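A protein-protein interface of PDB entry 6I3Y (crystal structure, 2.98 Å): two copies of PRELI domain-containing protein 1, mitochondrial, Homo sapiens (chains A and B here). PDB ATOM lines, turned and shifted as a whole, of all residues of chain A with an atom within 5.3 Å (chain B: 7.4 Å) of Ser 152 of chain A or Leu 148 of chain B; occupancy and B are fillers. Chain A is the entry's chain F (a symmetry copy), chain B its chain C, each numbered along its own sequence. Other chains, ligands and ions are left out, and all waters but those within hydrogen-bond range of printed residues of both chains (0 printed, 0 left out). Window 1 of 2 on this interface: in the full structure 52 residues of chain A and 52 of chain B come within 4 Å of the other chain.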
ATOM      1  N   LEU A 148       2.022 -12.892 -25.832  1.00  0.00           N
ATOM      2  CA  LEU A 148       0.591 -13.041 -25.993  1.00  0.00           C
ATOM      3  C   LEU A 148      -0.153 -11.728 -26.136  1.00  0.00           C
ATOM      4  O   LEU A 148      -1.136 -11.670 -26.863  1.00  0.00           O
ATOM      5  CB  LEU A 148      -0.001 -13.860 -24.857  1.00  0.00           C
ATOM      6  CG  LEU A 148       0.161 -15.354 -25.026  1.00  0.00           C
ATOM      7  CD1 LEU A 148       1.636 -15.739 -25.026  1.00  0.00           C
ATOM      8  CD2 LEU A 148      -0.623 -16.058 -23.925  1.00  0.00           C
ATOM      9  N   PHE A 149       0.318 -10.677 -25.481  1.00  0.00           N
ATOM     10  CA  PHE A 149      -0.304  -9.355 -25.652  1.00  0.00           C
ATOM     11  C   PHE A 149      -0.263  -8.925 -27.103  1.00  0.00           C
ATOM     12  O   PHE A 149      -1.262  -8.425 -27.623  1.00  0.00           O
ATOM     13  CB  PHE A 149       0.380  -8.283 -24.794  1.00  0.00           C
ATOM     14  CG  PHE A 149       0.005  -8.342 -23.350  1.00  0.00           C
ATOM     15  CD1 PHE A 149      -1.254  -7.894 -22.931  1.00  0.00           C
ATOM     16  CD2 PHE A 149       0.879  -8.882 -22.404  1.00  0.00           C
ATOM     17  CE1 PHE A 149      -1.627  -7.965 -21.595  1.00  0.00           C
ATOM     18  CE2 PHE A 149       0.498  -8.969 -21.073  1.00  0.00           C
ATOM     19  CZ  PHE A 149      -0.751  -8.500 -20.665  1.00  0.00           C
ATOM     20  N   GLY A 150       0.882  -9.122 -27.752  1.00  0.00           N
ATOM     21  CA  GLY A 150       1.035  -8.761 -29.152  1.00  0.00           C
ATOM     22  C   GLY A 150       0.069  -9.510 -30.053  1.00  0.00           C
ATOM     23  O   GLY A 150      -0.589  -8.905 -30.913  1.00  0.00           O
ATOM     24  N   VAL A 151      -0.045 -10.810 -29.839  1.00  0.00           N
ATOM     25  CA  VAL A 151      -0.932 -11.616 -30.675  1.00  0.00           C
ATOM     26  C   VAL A 151      -2.376 -11.204 -30.418  1.00  0.00           C
ATOM     27  O   VAL A 151      -3.149 -11.072 -31.359  1.00  0.00           O
ATOM     28  CB  VAL A 151      -0.769 -13.137 -30.463  1.00  0.00           C
ATOM     29  CG1 VAL A 151       0.678 -13.492 -30.147  1.00  0.00           C
ATOM     30  CG2 VAL A 151      -1.694 -13.663 -29.364  1.00  0.00           C
ATOM     31  N   SER A 152      -2.742 -10.972 -29.153  1.00  0.00           N
ATOM     32  CA  SER A 152      -4.101 -10.541 -28.843  1.00  0.00           C
ATOM     33  C   SER A 152      -4.413  -9.344 -29.726  1.00  0.00           C
ATOM     34  O   SER A 152      -5.511  -9.251 -30.249  1.00  0.00           O
ATOM     35  CB  SER A 152      -4.289 -10.164 -27.377  1.00  0.00           C
ATOM     36  OG  SER A 152      -3.794 -11.165 -26.499  1.00  0.00           O
ATOM     37  N   ARG A 153      -3.440  -8.458 -29.934  1.00  0.00           N
ATOM     38  CA  ARG A 153      -3.633  -7.363 -30.891  1.00  0.00           C
ATOM     39  C   ARG A 153      -3.696  -7.848 -32.341  1.00  0.00           C
ATOM     40  O   ARG A 153      -4.631  -7.479 -33.059  1.00  0.00           O
ATOM     41  CB  ARG A 153      -2.605  -6.249 -30.709  1.00  0.00           C
ATOM     42  CG  ARG A 153      -2.987  -5.318 -29.559  1.00  0.00           C
ATOM     43  CD  ARG A 153      -2.659  -3.850 -29.802  1.00  0.00           C
ATOM     44  NE  ARG A 153      -1.205  -3.583 -29.812  1.00  0.00           N
ATOM     45  CZ  ARG A 153      -0.586  -2.522 -29.272  1.00  0.00           C
ATOM     46  NH1 ARG A 153      -1.249  -1.572 -28.609  1.00  0.00           N
ATOM     47  NH2 ARG A 153       0.737  -2.419 -29.381  1.00  0.00           N
ATOM     48  N   ALA A 154      -2.761  -8.698 -32.764  1.00  0.00           N
ATOM     49  CA  ALA A 154      -2.841  -9.285 -34.127  1.00  0.00           C
ATOM     50  C   ALA A 154      -4.193  -9.956 -34.423  1.00  0.00           C
ATOM     51  O   ALA A 154      -4.843  -9.625 -35.402  1.00  0.00           O
ATOM     52  CB  ALA A 154      -1.717 -10.273 -34.370  1.00  0.00           C
ATOM     53  N   VAL A 155      -4.619 -10.863 -33.550  1.00  0.00           N
ATOM     54  CA  VAL A 155      -5.925 -11.514 -33.648  1.00  0.00           C
ATOM     55  C   VAL A 155      -7.042 -10.490 -33.712  1.00  0.00           C
ATOM     56  O   VAL A 155      -8.023 -10.717 -34.376  1.00  0.00           O
ATOM     57  CB  VAL A 155      -6.170 -12.478 -32.458  1.00  0.00           C
ATOM     58  CG1 VAL A 155      -7.635 -12.892 -32.326  1.00  0.00           C
ATOM     59  CG2 VAL A 155      -5.322 -13.729 -32.612  1.00  0.00           C
ATOM     60  N   GLN A 156      -6.911  -9.370 -33.017  1.00  0.00           N
ATOM     61  CA  GLN A 156      -7.899  -8.312 -33.129  1.00  0.00           C
ATOM     62  C   GLN A 156      -7.787  -7.570 -34.452  1.00  0.00           C
ATOM     63  O   GLN A 156      -8.801  -7.270 -35.069  1.00  0.00           O
ATOM     64  CB  GLN A 156      -7.751  -7.317 -31.996  1.00  0.00           C
ATOM     65  CG  GLN A 156      -9.078  -7.022 -31.339  1.00  0.00           C
ATOM     66  CD  GLN A 156      -8.926  -6.110 -30.171  1.00  0.00           C
ATOM     67  OE1 GLN A 156      -7.950  -5.361 -30.076  1.00  0.00           O
ATOM     68  NE2 GLN A 156      -9.887  -6.173 -29.259  1.00  0.00           N
ATOM     69  N   GLU A 157      -6.561  -7.255 -34.878  1.00  0.00           N
ATOM     70  CA  GLU A 157      -6.352  -6.517 -36.124  1.00  0.00           C
ATOM     71  C   GLU A 157      -6.861  -7.325 -37.316  1.00  0.00           C
ATOM     72  O   GLU A 157      -7.648  -6.840 -38.122  1.00  0.00           O
ATOM     73  CB  GLU A 157      -4.891  -6.137 -36.296  1.00  0.00           C
ATOM     74  N   MET B  13      -8.210  -2.300 -25.244  1.00  0.00           N
ATOM     75  CA  MET B  13      -9.031  -3.495 -24.925  1.00  0.00           C
ATOM     76  C   MET B  13      -9.884  -4.111 -26.044  1.00  0.00           C
ATOM     77  O   MET B  13      -9.499  -5.150 -26.568  1.00  0.00           O
ATOM     78  CB  MET B  13      -9.876  -3.173 -23.687  1.00  0.00           C
ATOM     79  CG  MET B  13     -10.631  -4.342 -23.088  1.00  0.00           C
ATOM     80  SD  MET B  13     -11.748  -3.784 -21.783  1.00  0.00           S
ATOM     81  CE  MET B  13     -12.408  -5.370 -21.246  1.00  0.00           C
ATOM     82  N   TRP B  77      -0.075 -17.618 -39.914  1.00  0.00           N
ATOM     83  CA  TRP B  77       0.493 -17.613 -38.579  1.00  0.00           C
ATOM     84  C   TRP B  77      -0.508 -18.031 -37.524  1.00  0.00           C
ATOM     85  O   TRP B  77      -0.123 -18.544 -36.489  1.00  0.00           O
ATOM     86  CB  TRP B  77       1.117 -16.255 -38.236  1.00  0.00           C
ATOM     87  CG  TRP B  77       0.153 -15.149 -38.189  1.00  0.00           C
ATOM     88  CD1 TRP B  77      -0.129 -14.295 -39.198  1.00  0.00           C
ATOM     89  CD2 TRP B  77      -0.685 -14.776 -37.087  1.00  0.00           C
ATOM     90  NE1 TRP B  77      -1.090 -13.393 -38.799  1.00  0.00           N
ATOM     91  CE2 TRP B  77      -1.449 -13.672 -37.507  1.00  0.00           C
ATOM     92  CE3 TRP B  77      -0.862 -15.262 -35.789  1.00  0.00           C
ATOM     93  CZ2 TRP B  77      -2.381 -13.050 -36.676  1.00  0.00           C
ATOM     94  CZ3 TRP B  77      -1.793 -14.645 -34.966  1.00  0.00           C
ATOM     95  CH2 TRP B  77      -2.536 -13.550 -35.411  1.00  0.00           C
ATOM     96  N   PHE B  82      -3.039 -21.453 -33.230  1.00  0.00           N
ATOM     97  CA  PHE B  82      -4.336 -22.013 -32.853  1.00  0.00           C
ATOM     98  C   PHE B  82      -4.671 -23.123 -33.830  1.00  0.00           C
ATOM     99  O   PHE B  82      -5.449 -22.930 -34.767  1.00  0.00           O
ATOM    100  CB  PHE B  82      -5.412 -20.921 -32.820  1.00  0.00           C
ATOM    101  CG  PHE B  82      -4.984 -19.694 -32.071  1.00  0.00           C
ATOM    102  CD1 PHE B  82      -5.100 -19.621 -30.694  1.00  0.00           C
ATOM    103  CD2 PHE B  82      -4.431 -18.626 -32.750  1.00  0.00           C
ATOM    104  CE1 PHE B  82      -4.656 -18.503 -30.014  1.00  0.00           C
ATOM    105  CE2 PHE B  82      -4.006 -17.505 -32.088  1.00  0.00           C
ATOM    106  CZ  PHE B  82      -4.107 -17.444 -30.717  1.00  0.00           C
ATOM    107  N   ALA B 115     -15.461 -18.331 -29.840  1.00  0.00           N
ATOM    108  CA  ALA B 115     -15.615 -17.305 -28.836  1.00  0.00           C
ATOM    109  C   ALA B 115     -14.295 -17.056 -28.112  1.00  0.00           C
ATOM    110  O   ALA B 115     -13.947 -15.912 -27.858  1.00  0.00           O
ATOM    111  CB  ALA B 115     -16.692 -17.724 -27.843  1.00  0.00           C
ATOM    112  N   ARG B 116     -13.575 -18.136 -27.799  1.00  0.00           N
ATOM    113  CA  ARG B 116     -12.265 -18.067 -27.149  1.00  0.00           C
ATOM    114  C   ARG B 116     -11.433 -16.945 -27.732  1.00  0.00           C
ATOM    115  O   ARG B 116     -11.148 -15.934 -27.063  1.00  0.00           O
ATOM    116  CB  ARG B 116     -11.490 -19.388 -27.325  1.00  0.00           C
ATOM    117  CG  ARG B 116     -12.114 -20.608 -26.677  1.00  0.00           C
ATOM    118  CD  ARG B 116     -12.084 -20.565 -25.151  1.00  0.00           C
ATOM    119  NE  ARG B 116     -13.275 -21.182 -24.550  1.00  0.00           N
ATOM    120  CZ  ARG B 116     -13.615 -22.473 -24.637  1.00  0.00           C
ATOM    121  NH1 ARG B 116     -12.867 -23.359 -25.305  1.00  0.00           N
ATOM    122  NH2 ARG B 116     -14.737 -22.885 -24.047  1.00  0.00           N
ATOM    123  N   LEU B 117     -11.087 -17.099 -29.003  1.00  0.00           N
ATOM    124  CA  LEU B 117     -10.047 -16.271 -29.560  1.00  0.00           C
ATOM    125  C   LEU B 117     -10.556 -14.961 -30.132  1.00  0.00           C
ATOM    126  O   LEU B 117      -9.756 -14.071 -30.380  1.00  0.00           O
ATOM    127  CB  LEU B 117      -9.176 -17.041 -30.545  1.00  0.00           C
ATOM    128  CG  LEU B 117      -9.684 -17.266 -31.950  1.00  0.00           C
ATOM    129  CD1 LEU B 117      -8.495 -17.574 -32.843  1.00  0.00           C
ATOM    130  CD2 LEU B 117     -10.715 -18.381 -32.009  1.00  0.00           C
ATOM    131  N   MET B 118     -11.864 -14.823 -30.326  1.00  0.00           N
ATOM    132  CA  MET B 118     -12.418 -13.577 -30.861  1.00  0.00           C
ATOM    133  C   MET B 118     -13.927 -13.551 -30.814  1.00  0.00           C
ATOM    134  O   MET B 118     -14.541 -14.561 -31.051  1.00  0.00           O
ATOM    135  CB  MET B 118     -12.021 -13.463 -32.315  1.00  0.00           C
ATOM    136  CG  MET B 118     -12.203 -12.102 -32.911  1.00  0.00           C
ATOM    137  SD  MET B 118     -10.875 -11.875 -34.095  1.00  0.00           S
ATOM    138  CE  MET B 118     -11.379 -12.900 -35.448  1.00  0.00           C
ATOM    139  N   SER B 145     -13.494  -7.981 -30.148  1.00  0.00           N
ATOM    140  CA  SER B 145     -12.761  -8.268 -28.923  1.00  0.00           C
ATOM    141  C   SER B 145     -12.131  -9.652 -29.012  1.00  0.00           C
ATOM    142  O   SER B 145     -12.253 -10.338 -30.037  1.00  0.00           O
ATOM    143  CB  SER B 145     -13.691  -8.168 -27.730  1.00  0.00           C
ATOM    144  OG  SER B 145     -14.506  -9.300 -27.620  1.00  0.00           O
ATOM    145  N   SER B 146     -11.449 -10.047 -27.938  1.00  0.00           N
ATOM    146  CA  SER B 146     -10.797 -11.362 -27.846  1.00  0.00           C
ATOM    147  C   SER B 146     -10.467 -11.675 -26.403  1.00  0.00           C
ATOM    148  O   SER B 146      -9.749 -10.894 -25.752  1.00  0.00           O
ATOM    149  CB  SER B 146      -9.493 -11.372 -28.643  1.00  0.00           C
ATOM    150  OG  SER B 146      -8.843 -12.620 -28.528  1.00  0.00           O
ATOM    151  N   SER B 147     -10.945 -12.820 -25.914  1.00  0.00           N
ATOM    152  CA  SER B 147     -10.679 -13.234 -24.510  1.00  0.00           C
ATOM    153  C   SER B 147      -9.183 -13.429 -24.211  1.00  0.00           C
ATOM    154  O   SER B 147      -8.771 -13.448 -23.049  1.00  0.00           O
ATOM    155  CB  SER B 147     -11.423 -14.529 -24.140  1.00  0.00           C
ATOM    156  OG  SER B 147     -10.511 -15.598 -23.900  1.00  0.00           O
ATOM    157  N   LEU B 148      -8.411 -13.618 -25.280  1.00  0.00           N
ATOM    158  CA  LEU B 148      -6.951 -13.733 -25.266  1.00  0.00           C
ATOM    159  C   LEU B 148      -6.151 -12.595 -24.600  1.00  0.00           C
ATOM    160  O   LEU B 148      -4.989 -12.787 -24.296  1.00  0.00           O
ATOM    161  CB  LEU B 148      -6.477 -13.872 -26.712  1.00  0.00           C
ATOM    162  CG  LEU B 148      -5.421 -14.902 -27.053  1.00  0.00           C
ATOM    163  CD1 LEU B 148      -5.532 -15.154 -28.542  1.00  0.00           C
ATOM    164  CD2 LEU B 148      -3.999 -14.475 -26.709  1.00  0.00           C
ATOM    165  N   PHE B 149      -6.736 -11.413 -24.397  1.00  0.00           N
ATOM    166  CA  PHE B 149      -6.096 -10.379 -23.554  1.00  0.00           C
ATOM    167  C   PHE B 149      -6.074 -10.807 -22.100  1.00  0.00           C
ATOM    168  O   PHE B 149      -5.032 -10.826 -21.456  1.00  0.00           O
ATOM    169  CB  PHE B 149      -6.813  -9.052 -23.677  1.00  0.00           C
ATOM    170  CG  PHE B 149      -6.485  -8.319 -24.935  1.00  0.00           C
ATOM    171  CD1 PHE B 149      -5.309  -7.578 -25.023  1.00  0.00           C
ATOM    172  CD2 PHE B 149      -7.333  -8.373 -26.044  1.00  0.00           C
ATOM    173  CE1 PHE B 149      -4.987  -6.890 -26.190  1.00  0.00           C
ATOM    174  CE2 PHE B 149      -7.024  -7.683 -27.202  1.00  0.00           C
ATOM    175  CZ  PHE B 149      -5.848  -6.942 -27.276  1.00  0.00           C
ATOM    176  N   GLY B 150      -7.232 -11.183 -21.583  1.00  0.00           N
ATOM    177  CA  GLY B 150      -7.311 -11.700 -20.222  1.00  0.00           C
ATOM    178  C   GLY B 150      -6.302 -12.805 -19.958  1.00  0.00           C
ATOM    179  O   GLY B 150      -5.698 -12.874 -18.889  1.00  0.00           O
ATOM    180  N   VAL B 151      -6.125 -13.662 -20.952  1.00  0.00           N
ATOM    181  CA  VAL B 151      -5.199 -14.770 -20.853  1.00  0.00           C
ATOM    182  C   VAL B 151      -3.793 -14.254 -20.656  1.00  0.00           C
ATOM    183  O   VAL B 151      -3.088 -14.666 -19.737  1.00  0.00           O
ATOM    184  CB  VAL B 151      -5.260 -15.673 -22.108  1.00  0.00           C
ATOM    185  CG1 VAL B 151      -3.976 -16.466 -22.300  1.00  0.00           C
ATOM    186  CG2 VAL B 151      -6.441 -16.628 -22.010  1.00  0.00           C
ATOM    187  N   SER B 152      -3.372 -13.363 -21.532  1.00  0.00           N
ATOM    188  CA  SER B 152      -2.009 -12.874 -21.446  1.00  0.00           C
ATOM    189  C   SER B 152      -1.770 -12.148 -20.132  1.00  0.00           C
ATOM    190  O   SER B 152      -0.649 -12.145 -19.650  1.00  0.00           O
ATOM    191  CB  SER B 152      -1.623 -12.015 -22.659  1.00  0.00           C
ATOM    192  OG  SER B 152      -1.981 -10.679 -22.496  1.00  0.00           O
ATOM    193  N   ARG B 153      -2.814 -11.543 -19.565  1.00  0.00           N
ATOM    194  CA  ARG B 153      -2.738 -11.025 -18.196  1.00  0.00           C
ATOM    195  C   ARG B 153      -2.478 -12.173 -17.198  1.00  0.00           C
ATOM    196  O   ARG B 153      -1.576 -12.094 -16.377  1.00  0.00           O
ATOM    197  CB  ARG B 153      -4.022 -10.269 -17.802  1.00  0.00           C
ATOM    198  CG  ARG B 153      -3.871  -8.776 -17.557  1.00  0.00           C
ATOM    199  CD  ARG B 153      -5.044  -8.260 -16.724  1.00  0.00           C
ATOM    200  N   ALA B 154      -3.273 -13.238 -17.280  1.00  0.00           N
ATOM    201  CA  ALA B 154      -3.130 -14.396 -16.387  1.00  0.00           C
ATOM    202  C   ALA B 154      -1.731 -14.968 -16.428  1.00  0.00           C
ATOM    203  O   ALA B 154      -1.172 -15.252 -15.373  1.00  0.00           O
ATOM    204  CB  ALA B 154      -4.135 -15.486 -16.740  1.00  0.00           C
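O of Met 13 of chain B lies within hydrogen-bond range of NE2 of Gln 156 of chain A (2.9 Å). OG of Ser 152 of chain A lies within hydrogen-bond range of O of Leu 148 of chain B. The backbone carbonyl oxygen (O) of Val 155 of chain A lies close to the side-chain sulfur (SD) of Met 118 of chain B, 3.1 Å away.
The backbone carbonyl oxygen of Leu 117 of chain B lies within hydrogen-bond range of the side-chain hydroxyl of Ser 146 of chain B. The side-chain hydroxyl (OG) of Ser 146 of chain B lies close to the backbone NH (N) of Leu 148 of chain B (3.4 Å). The backbone carbonyl oxygen (O) of Phe 149 of chain B sits at hydrogen-bond distance from the side-chain hydroxyl (OG) of Ser 152 of chain B, at 3.2 Å. The backbone carbonyl oxygen of Leu 148 of chain A lies within hydrogen-bond range of the side-chain hydroxyl of Ser 152 of chain A (2.7 Å).
Among the printed residues, pairs that only touch across the chains: Phe 149 of chain A with Ser 152 of chain B, Val 155 of chain A with Leu 117 of chain B, Leu 148 of chain A with Ser 152 of chain B, Ala 154 of chain A with Trp 77 of chain B, Ser 152 of chain A with Phe 149 of chain B, Gln 156 of chain A with Ser 145 of chain B, Val 151 of chain A with Leu 148 of chain B, Leu 148 of chain A with Val 151 of chain B, Gln 156 of chain A with Phe 149 of chain B, Phe 149 of chain A with Arg 153 of chain B, Val 155 of chain A with Trp 77 of chain B, Arg 153 of chain A with Phe 149 of chain B and Val 155 of chain A with Ser 146 of chain B.
Ser 152 of chain A touches just these residues of chain B: Leu 148 (3.0 Å) and Phe 149 (3.6 Å). Of the printed residues of chain B, Gln 156 of chain A touches Met 13, Ser 145 and Phe 149. Of the printed residues of chain B, Arg 153 of chain A touches Phe 149 (3.9 Å). Printed residues of chain B within 4 Å of Ala 154 of chain A: Trp 77. Of the printed residues of chain B, Leu 148 of chain A touches Val 151 and Ser 152. Ser 147 of chain B touches none of the printed residues of chain A.
Of the 17 printed residues of chain B, 11 touch a printed residue of chain A. Printed residues of chain B that touch a printed residue of chain A: Met 13, Trp 77, Leu 117, Met 118, Ser 145, Ser 146, Leu 148, Phe 149, Val 151, Ser 152 and Arg 153. Of the 10 printed residues of chain A, 8 touch a printed residue of chain B. Along chain A the printed residues that touch a printed residue of chain B span positions 148 to 156. Among the printed residues, no Asp or Glu carboxylate lies within 4 Å of a Lys or Arg side-chain nitrogen of the other chain.
Leu 148 of chain A touches Val 151 of chain B, and with the chains exchanged Val 151 of chain A touches Leu 148 of chain B. Leu 148 of chain A touches Ser 152 of chain B, and with the chains exchanged Ser 152 of chain A touches Leu 148 of chain B. Phe 149 of chain A touches Ser 152 of chain B, and with the chains exchanged Ser 152 of chain A touches Phe 149 of chain B. Phe 149 of chain A touches Arg 153 of chain B, and with the chains exchanged Arg 153 of chain A touches Phe 149 of chain B.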
